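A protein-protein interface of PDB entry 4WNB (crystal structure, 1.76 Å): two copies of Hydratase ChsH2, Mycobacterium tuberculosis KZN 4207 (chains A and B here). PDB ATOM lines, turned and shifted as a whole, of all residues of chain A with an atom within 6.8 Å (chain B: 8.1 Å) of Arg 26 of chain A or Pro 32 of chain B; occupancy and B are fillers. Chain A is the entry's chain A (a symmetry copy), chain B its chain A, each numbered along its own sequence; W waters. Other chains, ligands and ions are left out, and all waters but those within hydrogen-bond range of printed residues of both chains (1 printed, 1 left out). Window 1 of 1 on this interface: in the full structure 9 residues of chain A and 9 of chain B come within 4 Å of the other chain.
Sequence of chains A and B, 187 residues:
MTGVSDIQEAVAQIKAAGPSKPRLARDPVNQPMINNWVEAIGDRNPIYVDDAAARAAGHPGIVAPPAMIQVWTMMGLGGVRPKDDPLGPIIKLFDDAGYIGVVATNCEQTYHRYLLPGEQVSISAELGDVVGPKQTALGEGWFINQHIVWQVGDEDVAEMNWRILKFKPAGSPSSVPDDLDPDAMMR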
ATOM      1  N   ARG A  23      -6.576 -29.043  18.185  1.00  0.00           N
ATOM      2  CA  ARG A  23      -5.409 -28.678  17.415  1.00  0.00           C
ATOM      3  C   ARG A  23      -5.860 -27.730  16.309  1.00  0.00           C
ATOM      4  O   ARG A  23      -6.772 -28.051  15.554  1.00  0.00           O
ATOM      5  CB  ARG A  23      -4.742 -29.932  16.853  1.00  0.00           C
ATOM      6  CG  ARG A  23      -3.643 -29.656  15.851  1.00  0.00           C
ATOM      7  CD  ARG A  23      -2.902 -30.932  15.499  1.00  0.00           C
ATOM      8  NE  ARG A  23      -3.743 -31.974  14.906  1.00  0.00           N
ATOM      9  CZ  ARG A  23      -4.096 -32.008  13.619  1.00  0.00           C
ATOM     10  NH1 ARG A  23      -3.718 -31.037  12.802  1.00  0.00           N
ATOM     11  NH2 ARG A  23      -4.845 -32.997  13.153  1.00  0.00           N
ATOM     12  N   LEU A  24      -5.237 -26.555  16.235  1.00  0.00           N
ATOM     13  CA  LEU A  24      -5.597 -25.548  15.237  1.00  0.00           C
ATOM     14  C   LEU A  24      -5.109 -25.888  13.830  1.00  0.00           C
ATOM     15  O   LEU A  24      -3.986 -26.355  13.646  1.00  0.00           O
ATOM     16  CB  LEU A  24      -5.043 -24.179  15.645  1.00  0.00           C
ATOM     17  CG  LEU A  24      -5.828 -23.366  16.679  1.00  0.00           C
ATOM     18  CD1 LEU A  24      -5.633 -23.891  18.099  1.00  0.00           C
ATOM     19  CD2 LEU A  24      -5.451 -21.892  16.583  1.00  0.00           C
ATOM     20  N   ALA A  25      -5.962 -25.638  12.842  1.00  0.00           N
ATOM     21  CA  ALA A  25      -5.598 -25.771  11.430  1.00  0.00           C
ATOM     22  C   ALA A  25      -4.418 -24.858  11.094  1.00  0.00           C
ATOM     23  O   ALA A  25      -4.293 -23.771  11.674  1.00  0.00           O
ATOM     24  CB  ALA A  25      -6.790 -25.431  10.553  1.00  0.00           C
ATOM     25  N   ARG A  26      -3.553 -25.286  10.178  1.00  0.00           N
ATOM     26  CA  ARG A  26      -2.405 -24.463   9.774  1.00  0.00           C
ATOM     27  C   ARG A  26      -2.840 -23.061   9.354  1.00  0.00           C
ATOM     28  O   ARG A  26      -2.230 -22.070   9.746  1.00  0.00           O
ATOM     29  CB  ARG A  26      -1.629 -25.095   8.615  1.00  0.00           C
ATOM     30  CG  ARG A  26      -0.241 -24.475   8.402  1.00  0.00           C
ATOM     31  CD  ARG A  26       0.404 -25.006   7.138  1.00  0.00           C
ATOM     32  NE  ARG A  26      -0.442 -24.683   5.995  1.00  0.00           N
ATOM     33  CZ  ARG A  26      -0.172 -25.017   4.738  1.00  0.00           C
ATOM     34  NH1 ARG A  26       0.924 -25.703   4.445  1.00  0.00           N
ATOM     35  NH2 ARG A  26      -1.015 -24.665   3.779  1.00  0.00           N
ATOM     36  N   ASP A  27      -3.890 -23.003   8.543  1.00  0.00           N
ATOM     37  CA  ASP A  27      -4.433 -21.751   8.031  1.00  0.00           C
ATOM     38  C   ASP A  27      -5.903 -21.647   8.348  1.00  0.00           C
ATOM     39  O   ASP A  27      -6.573 -22.667   8.494  1.00  0.00           O
ATOM     40  CB  ASP A  27      -4.281 -21.641   6.510  1.00  0.00           C
ATOM     41  CG  ASP A  27      -3.030 -22.287   6.000  1.00  0.00           C
ATOM     42  OD1 ASP A  27      -1.956 -21.652   6.050  1.00  0.00           O
ATOM     43  OD2 ASP A  27      -3.135 -23.438   5.537  1.00  0.00           O
ATOM     44  N   PRO A  28      -6.421 -20.406   8.393  1.00  0.00           N
ATOM     45  CA  PRO A  28      -7.870 -20.208   8.306  1.00  0.00           C
ATOM     46  C   PRO A  28      -8.419 -20.725   6.992  1.00  0.00           C
ATOM     47  O   PRO A  28      -7.649 -20.934   6.032  1.00  0.00           O
ATOM     48  CB  PRO A  28      -8.041 -18.676   8.384  1.00  0.00           C
ATOM     49  CG  PRO A  28      -6.737 -18.147   8.819  1.00  0.00           C
ATOM     50  CD  PRO A  28      -5.683 -19.134   8.441  1.00  0.00           C
ATOM     51  N   VAL A  29      -9.728 -20.934   6.947  1.00  0.00           N
ATOM     52  CA  VAL A  29     -10.407 -21.201   5.697  1.00  0.00           C
ATOM     53  C   VAL A  29      -9.972 -20.090   4.760  1.00  0.00           C
ATOM     54  O   VAL A  29      -9.999 -18.918   5.132  1.00  0.00           O
ATOM     55  CB  VAL A  29     -11.937 -21.243   5.862  1.00  0.00           C
ATOM     56  CG1 VAL A  29     -12.627 -21.392   4.515  1.00  0.00           C
ATOM     57  CG2 VAL A  29     -12.337 -22.392   6.816  1.00  0.00           C
ATOM     58  N   ASN A  30      -9.486 -20.444   3.584  1.00  0.00           N
ATOM     59  CA  ASN A  30      -8.930 -19.411   2.722  1.00  0.00           C
ATOM     60  C   ASN A  30      -9.182 -19.672   1.234  1.00  0.00           C
ATOM     61  O   ASN A  30      -9.303 -20.816   0.784  1.00  0.00           O
ATOM     62  CB  ASN A  30      -7.428 -19.244   2.999  1.00  0.00           C
ATOM     63  CG  ASN A  30      -6.595 -20.473   2.562  1.00  0.00           C
ATOM     64  OD1 ASN A  30      -6.219 -20.589   1.392  1.00  0.00           O
ATOM     65  ND2 ASN A  30      -6.293 -21.369   3.512  1.00  0.00           N
ATOM     66  N   GLN A  31      -9.280 -18.588   0.466  1.00  0.00           N
ATOM     67  CA  GLN A  31      -9.673 -18.716  -0.932  1.00  0.00           C
ATOM     68  C   GLN A  31      -8.642 -19.423  -1.812  1.00  0.00           C
ATOM     69  O   GLN A  31      -9.040 -20.168  -2.718  1.00  0.00           O
ATOM     70  CB  GLN A  31      -9.965 -17.342  -1.558  1.00  0.00           C
ATOM     71  CG  GLN A  31     -10.662 -17.479  -2.890  1.00  0.00           C
ATOM     72  CD  GLN A  31     -12.038 -18.072  -2.730  1.00  0.00           C
ATOM     73  OE1 GLN A  31     -12.775 -17.683  -1.822  1.00  0.00           O
ATOM     74  NE2 GLN A  31     -12.404 -19.011  -3.601  1.00  0.00           N
ATOM     75  N   PRO A  32      -7.336 -19.159  -1.596  1.00  0.00           N
ATOM     76  CA  PRO A  32      -6.384 -19.887  -2.447  1.00  0.00           C
ATOM     77  C   PRO A  32      -6.460 -21.413  -2.337  1.00  0.00           C
ATOM     78  O   PRO A  32      -6.342 -22.110  -3.353  1.00  0.00           O
ATOM     79  CB  PRO A  32      -5.033 -19.396  -1.938  1.00  0.00           C
ATOM     80  CG  PRO A  32      -5.311 -17.948  -1.563  1.00  0.00           C
ATOM     81  CD  PRO A  32      -6.662 -18.051  -0.883  1.00  0.00           C
ATOM     82  N   MET A  33      -6.647 -21.927  -1.136  1.00  0.00           N
ATOM     83  CA  MET A  33      -6.757 -23.382  -1.011  1.00  0.00           C
ATOM     84  C   MET A  33      -8.119 -23.883  -1.490  1.00  0.00           C
ATOM     85  O   MET A  33      -8.222 -24.993  -2.016  1.00  0.00           O
ATOM     86  CB  MET A  33      -6.479 -23.828   0.428  1.00  0.00           C
ATOM     87  CG  MET A  33      -5.010 -23.718   0.780  1.00  0.00           C
ATOM     88  SD  MET A  33      -4.713 -24.115   2.500  1.00  0.00           S
ATOM     89  CE  MET A  33      -5.709 -25.607   2.676  1.00  0.00           C
ATOM     90  N   TRP A  72      -8.458 -28.611   6.082  1.00  0.00           N
ATOM     91  CA  TRP A  72      -7.855 -27.510   6.833  1.00  0.00           C
ATOM     92  C   TRP A  72      -6.905 -28.015   7.925  1.00  0.00           C
ATOM     93  O   TRP A  72      -5.875 -27.396   8.184  1.00  0.00           O
ATOM     94  CB  TRP A  72      -8.951 -26.598   7.439  1.00  0.00           C
ATOM     95  CG  TRP A  72      -9.987 -26.191   6.433  1.00  0.00           C
ATOM     96  CD1 TRP A  72     -11.299 -26.545   6.412  1.00  0.00           C
ATOM     97  CD2 TRP A  72      -9.765 -25.404   5.252  1.00  0.00           C
ATOM     98  NE1 TRP A  72     -11.925 -25.998   5.314  1.00  0.00           N
ATOM     99  CE2 TRP A  72     -10.998 -25.298   4.583  1.00  0.00           C
ATOM    100  CE3 TRP A  72      -8.648 -24.768   4.714  1.00  0.00           C
ATOM    101  CZ2 TRP A  72     -11.139 -24.614   3.383  1.00  0.00           C
ATOM    102  CZ3 TRP A  72      -8.792 -24.072   3.531  1.00  0.00           C
ATOM    103  CH2 TRP A  72     -10.030 -23.994   2.881  1.00  0.00           C
ATOM    104  N   THR A  73      -7.232 -29.161   8.530  1.00  0.00           N
ATOM    105  CA  THR A  73      -6.468 -29.675   9.659  1.00  0.00           C
ATOM    106  C   THR A  73      -5.568 -30.883   9.330  1.00  0.00           C
ATOM    107  O   THR A  73      -5.041 -31.527  10.232  1.00  0.00           O
ATOM    108  CB  THR A  73      -7.429 -30.044  10.837  1.00  0.00           C
ATOM    109  OG1 THR A  73      -8.461 -30.922  10.382  1.00  0.00           O
ATOM    110  CG2 THR A  73      -8.113 -28.782  11.387  1.00  0.00           C
ATOM    111  N   MET A  74      -5.367 -31.177   8.043  1.00  0.00           N
ATOM    112  CA  MET A  74      -4.432 -32.226   7.654  1.00  0.00           C
ATOM    113  C   MET A  74      -3.049 -31.865   8.175  1.00  0.00           C
ATOM    114  O   MET A  74      -2.673 -30.692   8.194  1.00  0.00           O
ATOM    115  CB  MET A  74      -4.414 -32.417   6.121  1.00  0.00           C
ATOM    116  CG  MET A  74      -5.701 -33.017   5.598  1.00  0.00           C
ATOM    117  SD  MET A  74      -5.956 -34.723   6.118  1.00  0.00           S
ATOM    118  CE  MET A  74      -4.764 -35.477   4.989  1.00  0.00           C
ATOM    119  N   MET A  75      -2.314 -32.878   8.628  1.00  0.00           N
ATOM    120  CA  MET A  75      -0.987 -32.686   9.226  1.00  0.00           C
ATOM    121  C   MET A  75       0.040 -32.061   8.290  1.00  0.00           C
ATOM    122  O   MET A  75       0.931 -31.336   8.737  1.00  0.00           O
ATOM    123  CB  MET A  75      -0.435 -34.022   9.742  1.00  0.00           C
ATOM    124  CG  MET A  75      -1.147 -34.589  10.968  1.00  0.00           C
ATOM    125  SD  MET A  75      -1.069 -33.519  12.428  1.00  0.00           S
ATOM    126  CE  MET A  75       0.689 -33.224  12.553  1.00  0.00           C
ATOM    127  N   GLY A  76      -0.056 -32.347   6.995  1.00  0.00           N
ATOM    128  CA  GLY A  76       0.895 -31.780   6.063  1.00  0.00           C
ATOM    129  C   GLY A  76       2.103 -32.666   5.844  1.00  0.00           C
ATOM    130  O   GLY A  76       2.244 -33.736   6.451  1.00  0.00           O
ATOM    131  N   GLN A 120     -11.213 -19.912  11.416  1.00  0.00           N
ATOM    132  CA  GLN A 120     -10.180 -20.896  11.671  1.00  0.00           C
ATOM    133  C   GLN A 120     -10.708 -22.036  12.535  1.00  0.00           C
ATOM    134  O   GLN A 120     -11.334 -21.842  13.593  1.00  0.00           O
ATOM    135  CB  GLN A 120      -8.953 -20.269  12.325  1.00  0.00           C
ATOM    136  CG  GLN A 120      -7.720 -21.182  12.320  1.00  0.00           C
ATOM    137  CD  GLN A 120      -6.413 -20.403  12.377  1.00  0.00           C
ATOM    138  OE1 GLN A 120      -6.410 -19.190  12.590  1.00  0.00           O
ATOM    139  NE2 GLN A 120      -5.302 -21.093  12.180  1.00  0.00           N
ATOM    140  N   VAL A 121     -10.409 -23.234  12.055  1.00  0.00           N
ATOM    141  CA  VAL A 121     -10.971 -24.478  12.546  1.00  0.00           C
ATOM    142  C   VAL A 121      -9.984 -25.149  13.481  1.00  0.00           C
ATOM    143  O   VAL A 121      -8.768 -25.001  13.320  1.00  0.00           O
ATOM    144  CB  VAL A 121     -11.296 -25.420  11.340  1.00  0.00           C
ATOM    145  CG1 VAL A 121     -11.764 -26.771  11.794  1.00  0.00           C
ATOM    146  CG2 VAL A 121     -12.335 -24.769  10.425  1.00  0.00           C
ATOM    147  N   PRO B  28      -3.922 -12.970  -4.847  1.00  0.00           N
ATOM    148  CA  PRO B  28      -2.858 -12.152  -4.262  1.00  0.00           C
ATOM    149  C   PRO B  28      -1.788 -13.014  -3.624  1.00  0.00           C
ATOM    150  O   PRO B  28      -2.027 -14.208  -3.352  1.00  0.00           O
ATOM    151  CB  PRO B  28      -3.581 -11.320  -3.181  1.00  0.00           C
ATOM    152  CG  PRO B  28      -5.021 -11.489  -3.440  1.00  0.00           C
ATOM    153  CD  PRO B  28      -5.216 -12.772  -4.174  1.00  0.00           C
ATOM    154  N   VAL B  29      -0.623 -12.424  -3.392  1.00  0.00           N
ATOM    155  CA  VAL B  29       0.397 -13.058  -2.584  1.00  0.00           C
ATOM    156  C   VAL B  29      -0.304 -13.464  -1.302  1.00  0.00           C
ATOM    157  O   VAL B  29      -1.024 -12.663  -0.707  1.00  0.00           O
ATOM    158  CB  VAL B  29       1.589 -12.124  -2.312  1.00  0.00           C
ATOM    159  CG1 VAL B  29       2.579 -12.768  -1.354  1.00  0.00           C
ATOM    160  CG2 VAL B  29       2.279 -11.741  -3.641  1.00  0.00           C
ATOM    161  N   ASN B  30      -0.182 -14.722  -0.916  1.00  0.00           N
ATOM    162  CA  ASN B  30      -0.956 -15.176   0.230  1.00  0.00           C
ATOM    163  C   ASN B  30      -0.214 -16.210   1.084  1.00  0.00           C
ATOM    164  O   ASN B  30       0.627 -16.973   0.598  1.00  0.00           O
ATOM    165  CB  ASN B  30      -2.314 -15.726  -0.235  1.00  0.00           C
ATOM    166  CG  ASN B  30      -2.186 -17.038  -1.044  1.00  0.00           C
ATOM    167  OD1 ASN B  30      -2.107 -18.125  -0.464  1.00  0.00           O
ATOM    168  ND2 ASN B  30      -2.190 -16.930  -2.380  1.00  0.00           N
ATOM    169  N   GLN B  31      -0.524 -16.217   2.379  1.00  0.00           N
ATOM    170  CA  GLN B  31       0.232 -17.050   3.306  1.00  0.00           C
ATOM    171  C   GLN B  31       0.037 -18.552   3.103  1.00  0.00           C
ATOM    172  O   GLN B  31       1.002 -19.310   3.272  1.00  0.00           O
ATOM    173  CB  GLN B  31      -0.119 -16.721   4.766  1.00  0.00           C
ATOM    174  CG  GLN B  31       0.866 -17.346   5.725  1.00  0.00           C
ATOM    175  CD  GLN B  31       2.239 -16.745   5.569  1.00  0.00           C
ATOM    176  OE1 GLN B  31       2.368 -15.525   5.450  1.00  0.00           O
ATOM    177  NE2 GLN B  31       3.276 -17.581   5.569  1.00  0.00           N
ATOM    178  N   PRO B  32      -1.202 -18.995   2.799  1.00  0.00           N
ATOM    179  CA  PRO B  32      -1.331 -20.444   2.582  1.00  0.00           C
ATOM    180  C   PRO B  32      -0.467 -21.004   1.450  1.00  0.00           C
ATOM    181  O   PRO B  32       0.093 -22.101   1.587  1.00  0.00           O
ATOM    182  CB  PRO B  32      -2.808 -20.602   2.237  1.00  0.00           C
ATOM    183  CG  PRO B  32      -3.479 -19.538   3.093  1.00  0.00           C
ATOM    184  CD  PRO B  32      -2.533 -18.364   2.939  1.00  0.00           C
ATOM    185  N   MET B  33      -0.359 -20.280   0.352  1.00  0.00           N
ATOM    186  CA  MET B  33       0.490 -20.780  -0.731  1.00  0.00           C
ATOM    187  C   MET B  33       1.973 -20.599  -0.409  1.00  0.00           C
ATOM    188  O   MET B  33       2.802 -21.410  -0.825  1.00  0.00           O
ATOM    189  CB  MET B  33       0.129 -20.111  -2.061  1.00  0.00           C
ATOM    190  CG  MET B  33      -1.192 -20.615  -2.605  1.00  0.00           C
ATOM    191  SD  MET B  33      -1.672 -19.735  -4.090  1.00  0.00           S
ATOM    192  CE  MET B  33      -0.114 -19.731  -4.995  1.00  0.00           C
ATOM    193  N   ILE B  34       2.322 -19.539   0.319  1.00  0.00           N
ATOM    194  CA  ILE B  34       3.675 -19.461   0.841  1.00  0.00           C
ATOM    195  C   ILE B  34       3.980 -20.683   1.718  1.00  0.00           C
ATOM    196  O   ILE B  34       5.044 -21.301   1.593  1.00  0.00           O
ATOM    197  CB  ILE B  34       3.920 -18.200   1.678  1.00  0.00           C
ATOM    198  CG1 ILE B  34       3.898 -16.952   0.802  1.00  0.00           C
ATOM    199  CG2 ILE B  34       5.268 -18.299   2.356  1.00  0.00           C
ATOM    200  CD1 ILE B  34       3.969 -15.634   1.614  1.00  0.00           C
ATOM    201  N   ASN B  35       3.044 -21.026   2.605  1.00  0.00           N
ATOM    202  CA  ASN B  35       3.240 -22.182   3.467  1.00  0.00           C
ATOM    203  C   ASN B  35       3.450 -23.487   2.670  1.00  0.00           C
ATOM    204  O   ASN B  35       4.331 -24.284   3.003  1.00  0.00           O
ATOM    205  CB  ASN B  35       2.059 -22.351   4.436  1.00  0.00           C
ATOM    206  CG  ASN B  35       2.025 -21.279   5.503  1.00  0.00           C
ATOM    207  OD1 ASN B  35       3.044 -20.627   5.781  1.00  0.00           O
ATOM    208  ND2 ASN B  35       0.857 -21.091   6.120  1.00  0.00           N
ATOM    209  N   ASN B  36       2.631 -23.710   1.643  1.00  0.00           N
ATOM    210  CA  ASN B  36       2.785 -24.909   0.807  1.00  0.00           C
ATOM    211  C   ASN B  36       4.168 -24.955   0.185  1.00  0.00           C
ATOM    212  O   ASN B  36       4.786 -26.011   0.100  1.00  0.00           O
ATOM    213  CB  ASN B  36       1.726 -24.964  -0.310  1.00  0.00           C
ATOM    214  CG  ASN B  36       0.347 -25.272   0.215  1.00  0.00           C
ATOM    215  OD1 ASN B  36       0.206 -25.735   1.342  1.00  0.00           O
ATOM    216  ND2 ASN B  36      -0.677 -25.035  -0.605  1.00  0.00           N
ATOM    217  N   TRP B  37       4.641 -23.790  -0.253  1.00  0.00           N
ATOM    218  CA  TRP B  37       5.909 -23.717  -0.974  1.00  0.00           C
ATOM    219  C   TRP B  37       7.101 -23.939  -0.032  1.00  0.00           C
ATOM    220  O   TRP B  37       7.956 -24.772  -0.322  1.00  0.00           O
ATOM    221  CB  TRP B  37       6.004 -22.360  -1.706  1.00  0.00           C
ATOM    222  CG  TRP B  37       7.138 -22.157  -2.658  1.00  0.00           C
ATOM    223  CD1 TRP B  37       7.107 -22.301  -4.026  1.00  0.00           C
ATOM    224  CD2 TRP B  37       8.451 -21.682  -2.336  1.00  0.00           C
ATOM    225  NE1 TRP B  37       8.333 -21.957  -4.571  1.00  0.00           N
ATOM    226  CE2 TRP B  37       9.178 -21.592  -3.554  1.00  0.00           C
ATOM    227  CE3 TRP B  37       9.095 -21.351  -1.134  1.00  0.00           C
ATOM    228  CZ2 TRP B  37      10.515 -21.182  -3.599  1.00  0.00           C
ATOM    229  CZ3 TRP B  37      10.423 -20.949  -1.180  1.00  0.00           C
ATOM    230  CH2 TRP B  37      11.115 -20.862  -2.405  1.00  0.00           C
ATOM    231  N   VAL B  38       7.146 -23.238   1.105  1.00  0.00           N
ATOM    232  CA  VAL B  38       8.293 -23.384   2.005  1.00  0.00           C
ATOM    233  C   VAL B  38       8.299 -24.805   2.585  1.00  0.00           C
ATOM    234  O   VAL B  38       9.361 -25.401   2.792  1.00  0.00           O
ATOM    235  CB  VAL B  38       8.292 -22.307   3.137  1.00  0.00           C
ATOM    236  CG1 VAL B  38       8.369 -20.910   2.540  1.00  0.00           C
ATOM    237  CG2 VAL B  38       7.077 -22.435   4.011  1.00  0.00           C
ATOM    238  N   GLU B  39       7.109 -25.362   2.798  1.00  0.00           N
ATOM    239  CA  GLU B  39       6.954 -26.761   3.216  1.00  0.00           C
ATOM    240  C   GLU B  39       7.617 -27.748   2.240  1.00  0.00           C
ATOM    241  O   GLU B  39       8.370 -28.642   2.643  1.00  0.00           O
ATOM    242  CB  GLU B  39       5.456 -27.100   3.377  1.00  0.00           C
ATOM    243  CG  GLU B  39       5.107 -28.578   3.487  1.00  0.00           C
ATOM    244  CD  GLU B  39       3.596 -28.836   3.651  1.00  0.00           C
ATOM    245  OE1 GLU B  39       3.175 -29.243   4.756  1.00  0.00           O
ATOM    246  OE2 GLU B  39       2.827 -28.642   2.682  1.00  0.00           O
ATOM    247  N   ALA B  40       7.313 -27.597   0.958  1.00  0.00           N
ATOM    248  CA  ALA B  40       7.812 -28.530  -0.045  1.00  0.00           C
ATOM    249  C   ALA B  40       9.297 -28.290  -0.353  1.00  0.00           C
ATOM    250  O   ALA B  40      10.066 -29.252  -0.480  1.00  0.00           O
ATOM    251  CB  ALA B  40       6.982 -28.431  -1.303  1.00  0.00           C
ATOM    252  N   TYR B  48       9.484 -15.655   5.909  1.00  0.00           N
ATOM    253  CA  TYR B  48       8.348 -16.060   5.078  1.00  0.00           C
ATOM    254  C   TYR B  48       7.138 -16.493   5.913  1.00  0.00           C
ATOM    255  O   TYR B  48       6.024 -16.601   5.387  1.00  0.00           O
ATOM    256  CB  TYR B  48       8.743 -17.205   4.128  1.00  0.00           C
ATOM    257  CG  TYR B  48       9.989 -16.936   3.302  1.00  0.00           C
ATOM    258  CD1 TYR B  48      10.237 -15.668   2.774  1.00  0.00           C
ATOM    259  CD2 TYR B  48      10.926 -17.939   3.068  1.00  0.00           C
ATOM    260  CE1 TYR B  48      11.372 -15.420   2.035  1.00  0.00           C
ATOM    261  CE2 TYR B  48      12.056 -17.698   2.333  1.00  0.00           C
ATOM    262  CZ  TYR B  48      12.275 -16.432   1.825  1.00  0.00           C
ATOM    263  OH  TYR B  48      13.406 -16.191   1.092  1.00  0.00           O
ATOM    264  N   MET B  68       9.252 -17.128  -5.500  1.00  0.00           N
ATOM    265  CA  MET B  68       7.852 -17.491  -5.721  1.00  0.00           C
ATOM    266  C   MET B  68       7.183 -16.610  -6.788  1.00  0.00           C
ATOM    267  O   MET B  68       6.022 -16.831  -7.116  1.00  0.00           O
ATOM    268  CB  MET B  68       7.047 -17.411  -4.412  1.00  0.00           C
ATOM    269  CG  MET B  68       7.152 -18.663  -3.560  1.00  0.00           C
ATOM    270  SD  MET B  68       5.863 -18.720  -2.272  1.00  0.00           S
ATOM    271  CE  MET B  68       4.477 -19.299  -3.247  1.00  0.00           C
ATOM    272  N   TRP B  72       2.796 -17.154  -8.611  1.00  0.00           N
ATOM    273  CA  TRP B  72       1.516 -16.460  -8.482  1.00  0.00           C
ATOM    274  C   TRP B  72       0.745 -16.429  -9.806  1.00  0.00           C
ATOM    275  O   TRP B  72      -0.480 -16.533  -9.813  1.00  0.00           O
ATOM    276  CB  TRP B  72       1.725 -15.025  -7.937  1.00  0.00           C
ATOM    277  CG  TRP B  72       2.593 -14.990  -6.714  1.00  0.00           C
ATOM    278  CD1 TRP B  72       3.833 -14.446  -6.600  1.00  0.00           C
ATOM    279  CD2 TRP B  72       2.304 -15.599  -5.446  1.00  0.00           C
ATOM    280  NE1 TRP B  72       4.325 -14.638  -5.328  1.00  0.00           N
ATOM    281  CE2 TRP B  72       3.403 -15.351  -4.603  1.00  0.00           C
ATOM    282  CE3 TRP B  72       1.214 -16.306  -4.943  1.00  0.00           C
ATOM    283  CZ2 TRP B  72       3.463 -15.820  -3.298  1.00  0.00           C
ATOM    284  CZ3 TRP B  72       1.264 -16.756  -3.639  1.00  0.00           C
ATOM    285  CH2 TRP B  72       2.378 -16.505  -2.827  1.00  0.00           C
ATOM    286  N   PRO B 117       2.114 -10.364   1.533  1.00  0.00           N
ATOM    287  CA  PRO B 117       0.764 -10.934   1.484  1.00  0.00           C
ATOM    288  C   PRO B 117      -0.298  -9.863   1.235  1.00  0.00           C
ATOM    289  O   PRO B 117      -0.257  -8.796   1.846  1.00  0.00           O
ATOM    290  CB  PRO B 117       0.612 -11.568   2.867  1.00  0.00           C
ATOM    291  CG  PRO B 117       2.018 -12.022   3.192  1.00  0.00           C
ATOM    292  CD  PRO B 117       2.932 -10.950   2.604  1.00  0.00           C
HETATM  293  O   HOH W   1       3.019 -26.681   5.836  1.00  0.00           O
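Of the 18 printed residues of chain A, 5 touch a printed residue of chain B.
Printed residues of chain A that touch a printed residue of chain B: Arg 26, Asp 27, Asn 30, Pro 32 and Gly 76.
Along chain A the printed residues that touch a printed residue of chain B span positions 26 to 76.
Printed residues of chain B that touch a printed residue of chain A: Asn 30, Pro 32, Asn 35, Asn 36 and Glu 39.
Hydrophobic or aromatic side chains of chain B that line the printed part of chain A: Pro 32.
Among the printed residues, Asp or Glu carboxylates within 4 Å of a Lys or Arg side-chain nitrogen of the other chain: Arg 26 of chain A with Glu 39 of chain B (3.9 Å).
Asn 30 of chain A touches Pro 32 of chain B, and with the chains exchanged Pro 32 of chain A touches Asn 30 of chain B.
Positions printed for both chains: 28, 29, 30, 31, 32, 33 and 72.
Of the 9 pairs that touch across the chains among the printed residues, 2 have their exchanged pair printed and touching as well.
The side-chain amide nitrogen of Asn 30 of chain B lies within hydrogen-bond range of the backbone carbonyl oxygen of Pro 28 of chain B (2.9 Å).
The side-chain amide oxygen of Asn 30 of chain B lies within hydrogen-bond range of the backbone NH of Met 33 of chain B (2.9 Å).
The side-chain amide nitrogen (NE2) of Gln 31 of chain B is in hydrogen-bond range of the side-chain amide oxygen (OD1) of Asn 35 of chain B (3.1 Å).
The guanidinium group (NE) of Arg 26 of chain A lies within salt-bridge range of the side-chain carboxylate (OD2) of Asp 27 of chain A (3.0 Å).
O of Pro 28 of chain A sits at hydrogen-bond distance from ND2 of Asn 30 of chain A.
The backbone NH (N) of Met 33 of chain A is in hydrogen-bond range of the side-chain amide oxygen (OD1) of Asn 30 of chain A (2.9 Å).
Printed residues of chain B within 4 Å of Arg 26 of chain A: Pro 32, Asn 35, Asn 36 and Glu 39.
Printed residues of chain A within 4 Å of Pro 32 of chain B: Arg 26 (3.6 Å), Asp 27 (3.7 Å) and Asn 30 (3.3 Å).
No residue of chain B comes within 4 Å of Ala 25 of chain A.
Of chain B, only Pro 32 (3.7 Å) and Asn 35 (2.9 Å) come within 4 Å of Asp 27 of chain A.
Of the printed residues of chain B, Pro 32 of chain A touches Asn 30 (3.3 Å).
Of the printed residues of chain B, Asn 30 of chain A touches Pro 32.
Printed residues of chain A within 4 Å of Glu 39 of chain B: Arg 26 (3.9 Å) and Gly 76 (3.7 Å).
Of the printed residues of chain B, Gly 76 of chain A touches Glu 39 (3.7 Å).
Ile 34 of chain B touches none of the printed residues of chain A.
Met 74 of chain A touches none of the printed residues of chain B.
The nearest printed residue of chain A that does not touch Pro 32 of chain B is Met 33 of chain A (4.005 Å).
The nearest printed residue of chain A that does not touch Glu 39 of chain B is Met 75 of chain A (5.0 Å).
OD1 of Asp 27 of chain A lies within hydrogen-bond range of ND2 of Asn 35 of chain B (2.9 Å).
NH2 of Arg 26 of chain A sits at hydrogen-bond distance from OD1 of Asn 36 of chain B (2.9 Å).
The guanidinium group (NH1) of Arg 26 of chain A lies within salt-bridge range of the side-chain carboxylate (OE2) of Glu 39 of chain B, 3.9 Å away.
Water W1 bridges the guanidinium group (NH1) of Arg 26 of chain A and the side-chain carboxylate (OE1) of Glu 39 of chain B.
Pro 32 of chain B touches Arg 26 of chain A (O to NH2, 3.6 Å).
CB of Asn 35 of chain B touches CZ of Arg 26 of chain A, at 3.5 Å.
OD1 of Asp 27 of chain A touches CA of Pro 32 of chain B (3.7 Å).
Asn 30 of chain A touches Pro 32 of chain B.
Asn 30 of chain B touches Pro 32 of chain A.
CA of Gly 76 of chain A touches OE1 of Glu 39 of chain B, 3.7 Å away.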
